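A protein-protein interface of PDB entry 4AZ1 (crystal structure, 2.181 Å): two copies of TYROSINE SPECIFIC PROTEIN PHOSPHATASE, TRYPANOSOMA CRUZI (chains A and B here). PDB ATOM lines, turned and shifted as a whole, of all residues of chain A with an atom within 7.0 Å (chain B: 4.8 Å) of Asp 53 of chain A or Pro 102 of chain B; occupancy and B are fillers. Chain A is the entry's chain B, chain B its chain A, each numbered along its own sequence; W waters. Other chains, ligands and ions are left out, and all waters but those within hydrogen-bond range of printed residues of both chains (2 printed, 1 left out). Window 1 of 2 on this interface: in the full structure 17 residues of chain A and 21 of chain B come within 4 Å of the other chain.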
ATOM      1  N   ARG A  46      -9.500 -29.030 -35.496  1.00  0.00           N
ATOM      2  CA  ARG A  46      -9.716 -29.188 -34.060  1.00  0.00           C
ATOM      3  C   ARG A  46     -10.408 -30.520 -33.746  1.00  0.00           C
ATOM      4  O   ARG A  46     -10.074 -31.192 -32.772  1.00  0.00           O
ATOM      5  CB  ARG A  46     -10.572 -28.006 -33.553  1.00  0.00           C
ATOM      6  CG  ARG A  46     -10.176 -27.474 -32.179  1.00  0.00           C
ATOM      7  CD  ARG A  46      -8.780 -26.812 -32.176  1.00  0.00           C
ATOM      8  NE  ARG A  46      -8.324 -26.531 -30.807  1.00  0.00           N
ATOM      9  CZ  ARG A  46      -8.658 -25.446 -30.105  1.00  0.00           C
ATOM     10  NH1 ARG A  46      -9.456 -24.508 -30.636  1.00  0.00           N
ATOM     11  NH2 ARG A  46      -8.198 -25.300 -28.867  1.00  0.00           N
ATOM     12  N   ASN A  49      -8.036 -33.326 -33.157  1.00  0.00           N
ATOM     13  CA  ASN A  49      -7.008 -33.209 -32.111  1.00  0.00           C
ATOM     14  C   ASN A  49      -7.424 -33.926 -30.841  1.00  0.00           C
ATOM     15  O   ASN A  49      -8.565 -33.810 -30.415  1.00  0.00           O
ATOM     16  CB  ASN A  49      -6.713 -31.738 -31.794  1.00  0.00           C
ATOM     17  CG  ASN A  49      -6.031 -31.031 -32.937  1.00  0.00           C
ATOM     18  OD1 ASN A  49      -5.445 -31.671 -33.821  1.00  0.00           O
ATOM     19  ND2 ASN A  49      -6.108 -29.708 -32.939  1.00  0.00           N
ATOM     20  N   ARG A  50      -6.502 -34.648 -30.222  1.00  0.00           N
ATOM     21  CA  ARG A  50      -6.842 -35.384 -29.018  1.00  0.00           C
ATOM     22  C   ARG A  50      -7.007 -34.438 -27.828  1.00  0.00           C
ATOM     23  O   ARG A  50      -7.799 -34.703 -26.919  1.00  0.00           O
ATOM     24  CB  ARG A  50      -5.783 -36.457 -28.726  1.00  0.00           C
ATOM     25  CG  ARG A  50      -6.130 -37.314 -27.509  1.00  0.00           C
ATOM     26  CD  ARG A  50      -5.207 -38.522 -27.429  1.00  0.00           C
ATOM     27  NE  ARG A  50      -5.420 -39.414 -28.560  1.00  0.00           N
ATOM     28  CZ  ARG A  50      -6.388 -40.327 -28.611  1.00  0.00           C
ATOM     29  NH1 ARG A  50      -7.226 -40.445 -27.593  1.00  0.00           N
ATOM     30  NH2 ARG A  50      -6.523 -41.114 -29.676  1.00  0.00           N
ATOM     31  N   TYR A  51      -6.276 -33.325 -27.854  1.00  0.00           N
ATOM     32  CA  TYR A  51      -6.258 -32.407 -26.718  1.00  0.00           C
ATOM     33  C   TYR A  51      -6.535 -30.963 -27.134  1.00  0.00           C
ATOM     34  O   TYR A  51      -5.992 -30.489 -28.134  1.00  0.00           O
ATOM     35  CB  TYR A  51      -4.902 -32.511 -26.002  1.00  0.00           C
ATOM     36  CG  TYR A  51      -4.674 -33.854 -25.356  1.00  0.00           C
ATOM     37  CD1 TYR A  51      -5.354 -34.203 -24.191  1.00  0.00           C
ATOM     38  CD2 TYR A  51      -3.799 -34.783 -25.910  1.00  0.00           C
ATOM     39  CE1 TYR A  51      -5.155 -35.421 -23.587  1.00  0.00           C
ATOM     40  CE2 TYR A  51      -3.586 -36.028 -25.298  1.00  0.00           C
ATOM     41  CZ  TYR A  51      -4.271 -36.332 -24.142  1.00  0.00           C
ATOM     42  OH  TYR A  51      -4.111 -37.541 -23.515  1.00  0.00           O
ATOM     43  N   LEU A  52      -7.385 -30.275 -26.372  1.00  0.00           N
ATOM     44  CA  LEU A  52      -7.719 -28.873 -26.654  1.00  0.00           C
ATOM     45  C   LEU A  52      -6.478 -27.983 -26.743  1.00  0.00           C
ATOM     46  O   LEU A  52      -6.444 -27.027 -27.536  1.00  0.00           O
ATOM     47  CB  LEU A  52      -8.651 -28.339 -25.577  1.00  0.00           C
ATOM     48  CG  LEU A  52      -9.439 -27.068 -25.879  1.00  0.00           C
ATOM     49  CD1 LEU A  52     -10.363 -27.324 -27.061  1.00  0.00           C
ATOM     50  CD2 LEU A  52     -10.243 -26.656 -24.658  1.00  0.00           C
ATOM     51  N   ASP A  53      -5.452 -28.312 -25.953  1.00  0.00           N
ATOM     52  CA  ASP A  53      -4.297 -27.418 -25.795  1.00  0.00           C
ATOM     53  C   ASP A  53      -3.097 -27.786 -26.648  1.00  0.00           C
ATOM     54  O   ASP A  53      -2.081 -27.071 -26.623  1.00  0.00           O
ATOM     55  CB  ASP A  53      -3.873 -27.310 -24.314  1.00  0.00           C
ATOM     56  CG  ASP A  53      -3.528 -28.665 -23.691  1.00  0.00           C
ATOM     57  OD1 ASP A  53      -4.169 -29.678 -24.041  1.00  0.00           O
ATOM     58  OD2 ASP A  53      -2.618 -28.718 -22.830  1.00  0.00           O
ATOM     59  N   ILE A  54      -3.207 -28.886 -27.402  1.00  0.00           N
ATOM     60  CA  ILE A  54      -2.058 -29.393 -28.152  1.00  0.00           C
ATOM     61  C   ILE A  54      -2.220 -29.270 -29.672  1.00  0.00           C
ATOM     62  O   ILE A  54      -2.928 -30.068 -30.309  1.00  0.00           O
ATOM     63  CB  ILE A  54      -1.709 -30.862 -27.781  1.00  0.00           C
ATOM     64  CG1 ILE A  54      -1.528 -31.016 -26.260  1.00  0.00           C
ATOM     65  CG2 ILE A  54      -0.487 -31.329 -28.569  1.00  0.00           C
ATOM     66  CD1 ILE A  54      -0.485 -30.054 -25.603  1.00  0.00           C
ATOM     67  N   LEU A  55      -1.518 -28.290 -30.244  1.00  0.00           N
ATOM     68  CA  LEU A  55      -1.646 -27.922 -31.655  1.00  0.00           C
ATOM     69  C   LEU A  55      -0.314 -28.128 -32.394  1.00  0.00           C
ATOM     70  O   LEU A  55       0.755 -27.846 -31.845  1.00  0.00           O
ATOM     71  CB  LEU A  55      -2.059 -26.447 -31.751  1.00  0.00           C
ATOM     72  CG  LEU A  55      -3.341 -26.031 -31.038  1.00  0.00           C
ATOM     73  CD1 LEU A  55      -3.591 -24.515 -31.190  1.00  0.00           C
ATOM     74  CD2 LEU A  55      -4.539 -26.827 -31.564  1.00  0.00           C
ATOM     75  N   ALA A 228      -0.415 -37.207 -26.269  1.00  0.00           N
ATOM     76  CA  ALA A 228      -0.439 -35.862 -26.851  1.00  0.00           C
ATOM     77  C   ALA A 228       0.630 -35.690 -27.927  1.00  0.00           C
ATOM     78  O   ALA A 228       0.491 -34.853 -28.822  1.00  0.00           O
ATOM     79  CB  ALA A 228      -0.280 -34.804 -25.764  1.00  0.00           C
ATOM     80  N   ILE A 230       3.981 -34.993 -27.276  1.00  0.00           N
ATOM     81  CA  ILE A 230       5.038 -34.052 -26.918  1.00  0.00           C
ATOM     82  C   ILE A 230       5.902 -34.461 -25.700  1.00  0.00           C
ATOM     83  O   ILE A 230       7.071 -34.079 -25.614  1.00  0.00           O
ATOM     84  CB  ILE A 230       4.490 -32.614 -26.720  1.00  0.00           C
ATOM     85  CG1 ILE A 230       3.326 -32.611 -25.738  1.00  0.00           C
ATOM     86  CG2 ILE A 230       4.050 -31.988 -28.048  1.00  0.00           C
ATOM     87  CD1 ILE A 230       2.864 -31.209 -25.382  1.00  0.00           C
ATOM     88  N   PHE A 268       5.850 -27.331 -30.730  1.00  0.00           N
ATOM     89  CA  PHE A 268       5.650 -26.599 -29.486  1.00  0.00           C
ATOM     90  C   PHE A 268       5.444 -27.539 -28.294  1.00  0.00           C
ATOM     91  O   PHE A 268       4.589 -28.426 -28.343  1.00  0.00           O
ATOM     92  CB  PHE A 268       4.425 -25.689 -29.663  1.00  0.00           C
ATOM     93  CG  PHE A 268       4.250 -24.661 -28.579  1.00  0.00           C
ATOM     94  CD1 PHE A 268       4.952 -23.461 -28.621  1.00  0.00           C
ATOM     95  CD2 PHE A 268       3.351 -24.877 -27.538  1.00  0.00           C
ATOM     96  CE1 PHE A 268       4.773 -22.492 -27.633  1.00  0.00           C
ATOM     97  CE2 PHE A 268       3.168 -23.917 -26.541  1.00  0.00           C
ATOM     98  CZ  PHE A 268       3.886 -22.726 -26.588  1.00  0.00           C
ATOM     99  N   GLN A 272       7.543 -32.333 -21.814  1.00  0.00           N
ATOM    100  CA  GLN A 272       6.583 -31.558 -21.016  1.00  0.00           C
ATOM    101  C   GLN A 272       6.980 -31.306 -19.569  1.00  0.00           C
ATOM    102  O   GLN A 272       6.870 -30.182 -19.078  1.00  0.00           O
ATOM    103  CB  GLN A 272       5.212 -32.246 -20.999  1.00  0.00           C
ATOM    104  CG  GLN A 272       4.428 -32.178 -22.293  1.00  0.00           C
ATOM    105  CD  GLN A 272       3.024 -32.761 -22.146  1.00  0.00           C
ATOM    106  OE1 GLN A 272       2.804 -33.959 -22.365  1.00  0.00           O
ATOM    107  NE2 GLN A 272       2.072 -31.916 -21.767  1.00  0.00           N
ATOM    108  N   VAL B  98      -5.561 -20.390 -25.692  1.00  0.00           N
ATOM    109  CA  VAL B  98      -5.477 -21.847 -25.827  1.00  0.00           C
ATOM    110  C   VAL B  98      -4.399 -22.451 -24.923  1.00  0.00           C
ATOM    111  O   VAL B  98      -4.674 -23.372 -24.155  1.00  0.00           O
ATOM    112  CB  VAL B  98      -5.289 -22.267 -27.303  1.00  0.00           C
ATOM    113  CG1 VAL B  98      -4.894 -23.748 -27.420  1.00  0.00           C
ATOM    114  CG2 VAL B  98      -6.585 -22.001 -28.069  1.00  0.00           C
ATOM    115  N   GLN B  99      -3.197 -21.888 -24.963  1.00  0.00           N
ATOM    116  CA  GLN B  99      -2.106 -22.437 -24.163  1.00  0.00           C
ATOM    117  C   GLN B  99      -2.264 -22.133 -22.669  1.00  0.00           C
ATOM    118  O   GLN B  99      -1.529 -22.666 -21.840  1.00  0.00           O
ATOM    119  CB  GLN B  99      -0.747 -21.963 -24.685  1.00  0.00           C
ATOM    120  CG  GLN B  99      -0.516 -22.251 -26.177  1.00  0.00           C
ATOM    121  CD  GLN B  99      -0.489 -23.741 -26.537  1.00  0.00           C
ATOM    122  OE1 GLN B  99      -0.463 -24.617 -25.667  1.00  0.00           O
ATOM    123  NE2 GLN B  99      -0.487 -24.028 -27.838  1.00  0.00           N
ATOM    124  N   GLY B 100      -3.244 -21.303 -22.322  1.00  0.00           N
ATOM    125  CA  GLY B 100      -3.493 -20.967 -20.930  1.00  0.00           C
ATOM    126  C   GLY B 100      -4.725 -21.661 -20.372  1.00  0.00           C
ATOM    127  O   GLY B 100      -5.012 -21.575 -19.173  1.00  0.00           O
ATOM    128  N   ILE B 101      -5.457 -22.350 -21.241  1.00  0.00           N
ATOM    129  CA  ILE B 101      -6.642 -23.085 -20.802  1.00  0.00           C
ATOM    130  C   ILE B 101      -6.351 -24.175 -19.751  1.00  0.00           C
ATOM    131  O   ILE B 101      -7.133 -24.323 -18.809  1.00  0.00           O
ATOM    132  CB  ILE B 101      -7.466 -23.625 -21.994  1.00  0.00           C
ATOM    133  CG1 ILE B 101      -8.219 -22.479 -22.667  1.00  0.00           C
ATOM    134  CG2 ILE B 101      -8.472 -24.711 -21.557  1.00  0.00           C
ATOM    135  CD1 ILE B 101      -8.869 -22.882 -24.004  1.00  0.00           C
ATOM    136  N   PRO B 102      -5.230 -24.924 -19.892  1.00  0.00           N
ATOM    137  CA  PRO B 102      -5.002 -25.932 -18.850  1.00  0.00           C
ATOM    138  C   PRO B 102      -4.832 -25.280 -17.474  1.00  0.00           C
ATOM    139  O   PRO B 102      -5.324 -25.827 -16.471  1.00  0.00           O
ATOM    140  CB  PRO B 102      -3.693 -26.604 -19.285  1.00  0.00           C
ATOM    141  CG  PRO B 102      -3.609 -26.374 -20.764  1.00  0.00           C
ATOM    142  CD  PRO B 102      -4.242 -25.029 -20.987  1.00  0.00           C
ATOM    143  N   ASP B 103      -4.138 -24.142 -17.429  1.00  0.00           N
ATOM    144  CA  ASP B 103      -4.008 -23.365 -16.194  1.00  0.00           C
ATOM    145  C   ASP B 103      -5.374 -22.964 -15.651  1.00  0.00           C
ATOM    146  O   ASP B 103      -5.634 -23.032 -14.443  1.00  0.00           O
ATOM    147  CB  ASP B 103      -3.207 -22.094 -16.460  1.00  0.00           C
ATOM    148  CG  ASP B 103      -1.835 -22.381 -17.038  1.00  0.00           C
ATOM    149  OD1 ASP B 103      -1.758 -22.839 -18.211  1.00  0.00           O
ATOM    150  OD2 ASP B 103      -0.840 -22.136 -16.319  1.00  0.00           O
ATOM    151  N   PHE B 104      -6.245 -22.534 -16.549  1.00  0.00           N
ATOM    152  CA  PHE B 104      -7.547 -22.021 -16.145  1.00  0.00           C
ATOM    153  C   PHE B 104      -8.353 -23.160 -15.519  1.00  0.00           C
ATOM    154  O   PHE B 104      -8.911 -23.018 -14.421  1.00  0.00           O
ATOM    155  CB  PHE B 104      -8.257 -21.436 -17.364  1.00  0.00           C
ATOM    156  CG  PHE B 104      -9.625 -20.858 -17.078  1.00  0.00           C
ATOM    157  CD1 PHE B 104      -9.766 -19.687 -16.344  1.00  0.00           C
ATOM    158  CD2 PHE B 104     -10.765 -21.472 -17.576  1.00  0.00           C
ATOM    159  CE1 PHE B 104     -11.032 -19.146 -16.106  1.00  0.00           C
ATOM    160  CE2 PHE B 104     -12.035 -20.940 -17.336  1.00  0.00           C
ATOM    161  CZ  PHE B 104     -12.166 -19.780 -16.607  1.00  0.00           C
ATOM    162  N   LEU B 105      -8.387 -24.297 -16.205  1.00  0.00           N
ATOM    163  CA  LEU B 105      -9.152 -25.450 -15.729  1.00  0.00           C
ATOM    164  C   LEU B 105      -8.573 -25.994 -14.428  1.00  0.00           C
ATOM    165  O   LEU B 105      -9.315 -26.423 -13.526  1.00  0.00           O
ATOM    166  CB  LEU B 105      -9.206 -26.554 -16.795  1.00  0.00           C
ATOM    167  CG  LEU B 105      -9.901 -26.173 -18.111  1.00  0.00           C
ATOM    168  CD1 LEU B 105     -10.010 -27.365 -19.083  1.00  0.00           C
ATOM    169  CD2 LEU B 105     -11.265 -25.574 -17.868  1.00  0.00           C
ATOM    170  N   ALA B 106      -7.246 -25.988 -14.334  1.00  0.00           N
ATOM    171  CA  ALA B 106      -6.579 -26.467 -13.128  1.00  0.00           C
ATOM    172  C   ALA B 106      -6.952 -25.592 -11.938  1.00  0.00           C
ATOM    173  O   ALA B 106      -7.133 -26.086 -10.816  1.00  0.00           O
ATOM    174  CB  ALA B 106      -5.072 -26.475 -13.314  1.00  0.00           C
ATOM    175  N   ALA B 144     -10.297 -33.037 -23.241  1.00  0.00           N
ATOM    176  CA  ALA B 144      -9.192 -33.060 -22.277  1.00  0.00           C
ATOM    177  C   ALA B 144      -8.096 -32.034 -22.602  1.00  0.00           C
ATOM    178  O   ALA B 144      -7.945 -31.608 -23.760  1.00  0.00           O
ATOM    179  CB  ALA B 144      -8.606 -34.470 -22.176  1.00  0.00           C
ATOM    180  N   VAL B 145      -7.364 -31.608 -21.572  1.00  0.00           N
ATOM    181  CA  VAL B 145      -6.136 -30.850 -21.775  1.00  0.00           C
ATOM    182  C   VAL B 145      -4.977 -31.744 -21.372  1.00  0.00           C
ATOM    183  O   VAL B 145      -5.116 -32.624 -20.509  1.00  0.00           O
ATOM    184  CB  VAL B 145      -6.103 -29.507 -21.009  1.00  0.00           C
ATOM    185  CG1 VAL B 145      -7.096 -28.510 -21.614  1.00  0.00           C
ATOM    186  CG2 VAL B 145      -6.367 -29.715 -19.506  1.00  0.00           C
ATOM    187  N   SER B 146      -3.842 -31.558 -22.026  1.00  0.00           N
ATOM    188  CA  SER B 146      -2.691 -32.385 -21.730  1.00  0.00           C
ATOM    189  C   SER B 146      -1.827 -31.700 -20.670  1.00  0.00           C
ATOM    190  O   SER B 146      -1.156 -32.366 -19.873  1.00  0.00           O
ATOM    191  CB  SER B 146      -1.894 -32.632 -23.004  1.00  0.00           C
ATOM    192  OG  SER B 146      -0.698 -33.331 -22.714  1.00  0.00           O
ATOM    193  N   GLY B 147      -1.860 -30.367 -20.669  1.00  0.00           N
ATOM    194  CA  GLY B 147      -1.040 -29.571 -19.771  1.00  0.00           C
ATOM    195  C   GLY B 147      -1.382 -29.767 -18.307  1.00  0.00           C
ATOM    196  O   GLY B 147      -2.469 -30.243 -17.975  1.00  0.00           O
ATOM    197  N   ASN B 148      -0.446 -29.397 -17.434  1.00  0.00           N
ATOM    198  CA  ASN B 148      -0.649 -29.477 -15.991  1.00  0.00           C
ATOM    199  C   ASN B 148      -1.019 -30.883 -15.523  1.00  0.00           C
ATOM    200  O   ASN B 148      -1.907 -31.049 -14.686  1.00  0.00           O
ATOM    201  CB  ASN B 148      -1.712 -28.469 -15.537  1.00  0.00           C
ATOM    202  CG  ASN B 148      -1.291 -27.025 -15.769  1.00  0.00           C
ATOM    203  OD1 ASN B 148      -0.117 -26.681 -15.648  1.00  0.00           O
ATOM    204  ND2 ASN B 148      -2.249 -26.178 -16.103  1.00  0.00           N
ATOM    205  N   LEU B 151      -6.214 -32.701 -17.374  1.00  0.00           N
ATOM    206  CA  LEU B 151      -7.566 -32.632 -16.826  1.00  0.00           C
ATOM    207  C   LEU B 151      -8.545 -33.027 -17.916  1.00  0.00           C
ATOM    208  O   LEU B 151      -8.287 -32.829 -19.112  1.00  0.00           O
ATOM    209  CB  LEU B 151      -7.907 -31.228 -16.322  1.00  0.00           C
ATOM    210  CG  LEU B 151      -7.165 -30.653 -15.110  1.00  0.00           C
ATOM    211  CD1 LEU B 151      -6.204 -29.537 -15.515  1.00  0.00           C
ATOM    212  CD2 LEU B 151      -8.153 -30.143 -14.073  1.00  0.00           C
HETATM  213  O   HOH W   1      -1.836 -36.294 -22.038  1.00  0.00           O
HETATM  214  O   HOH W   2     -10.177 -33.433 -26.091  1.00  0.00           O
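Water W2 lies within hydrogen-bond range of the backbone carbonyl oxygen (O) of Arg 50 of chain A (2.8 Å) and the backbone NH (N) of Ala 144 of chain B (2.9 Å). Water W1 lies within hydrogen-bond range of the side-chain hydroxyl of Tyr 51 of chain A (3.0 Å) and the side-chain hydroxyl of Ser 146 of chain B (3.2 Å).
Among the printed residues, merely in contact across the chains: Asp 53 of chain A with Val 145 of chain B, Asp 53 of chain A with Pro 102 of chain B, Ala 228 of chain A with Ser 146 of chain B, Tyr 51 of chain A with Ala 144 of chain B, Leu 52 of chain A with Val 98 of chain B, Ile 54 of chain A with Ser 146 of chain B, Phe 268 of chain A with Gln 99 of chain B, Tyr 51 of chain A with Ser 146 of chain B, Arg 46 of chain A with Val 98 of chain B and Tyr 51 of chain A with Val 145 of chain B.
Printed residues of chain B within 4 Å of Arg 46 of chain A: Val 98. Of the printed residues of chain B, Leu 52 of chain A touches Val 98 and Ala 144. Of the printed residues of chain B, Asp 53 of chain A touches Gln 99, Pro 102, Val 145, Ser 146 and Gly 147. Of the printed residues of chain B, Ile 54 of chain A touches Ser 146 (3.7 Å). Of the printed residues of chain B, Phe 268 of chain A touches Gln 99 (3.7 Å). Pro 102 of chain B touches one residue of chain A. Leu 105 of chain B touches none of the printed residues of chain A. Ala 106 of chain B touches none of the printed residues of chain A. Of the printed residues of chain A, Gly 147 of chain B touches Asp 53 (2.8 Å).
ND2 of Asn 148 of chain B sits close to O of Pro 102 of chain B (3.1 Å). The backbone NH (N) of Val 145 of chain B is in hydrogen-bond range of the backbone carbonyl oxygen (O) of Leu 151 of chain B, 2.9 Å away. The guanidinium group (NH2) of Arg 46 of chain A is in hydrogen-bond range of the backbone carbonyl oxygen (O) of Leu 52 of chain A (2.8 Å).
No position is printed for both chains. Of the 15 pairs that touch across the chains among the printed residues, none has its exchanged pair printed and touching as well.
Of the 12 printed residues of chain A, 8 touch a printed residue of chain B. Printed residues of chain A that touch a printed residue of chain B: Arg 46, Tyr 51, Leu 52, Asp 53, Ile 54, Ala 228, Phe 268 and Gln 272. Of the 15 printed residues of chain B, 7 touch a printed residue of chain A. Hydrophobic or aromatic side chains of chain B that line the printed part of chain A: Val 98, Pro 102, Ala 144 and Val 145. Among the printed residues, 15 pairs touch across the chains. Among the printed residues, no Asp or Glu carboxylate lies within 4 Å of a Lys or Arg side-chain nitrogen of the other chain.
The side-chain amide oxygen of Gln 99 of chain B lies close to the backbone carbonyl oxygen of Asp 53 of chain A, 3.1 Å away. The backbone carbonyl oxygen of Ala 144 of chain B lies within hydrogen-bond range of the backbone NH of Leu 52 of chain A (3.0 Å). The backbone NH (N) of Ser 146 of chain B is in hydrogen-bond range of the side-chain carboxylate (OD1) of Asp 53 of chain A, at 2.8 Å. The side-chain amide nitrogen (NE2) of Gln 272 of chain A is in hydrogen-bond range of the side-chain hydroxyl (OG) of Ser 146 of chain B, at 3.3 Å. OD2 of Asp 53 of chain A sits at hydrogen-bond distance from N of Gly 147 of chain B (2.8 Å).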
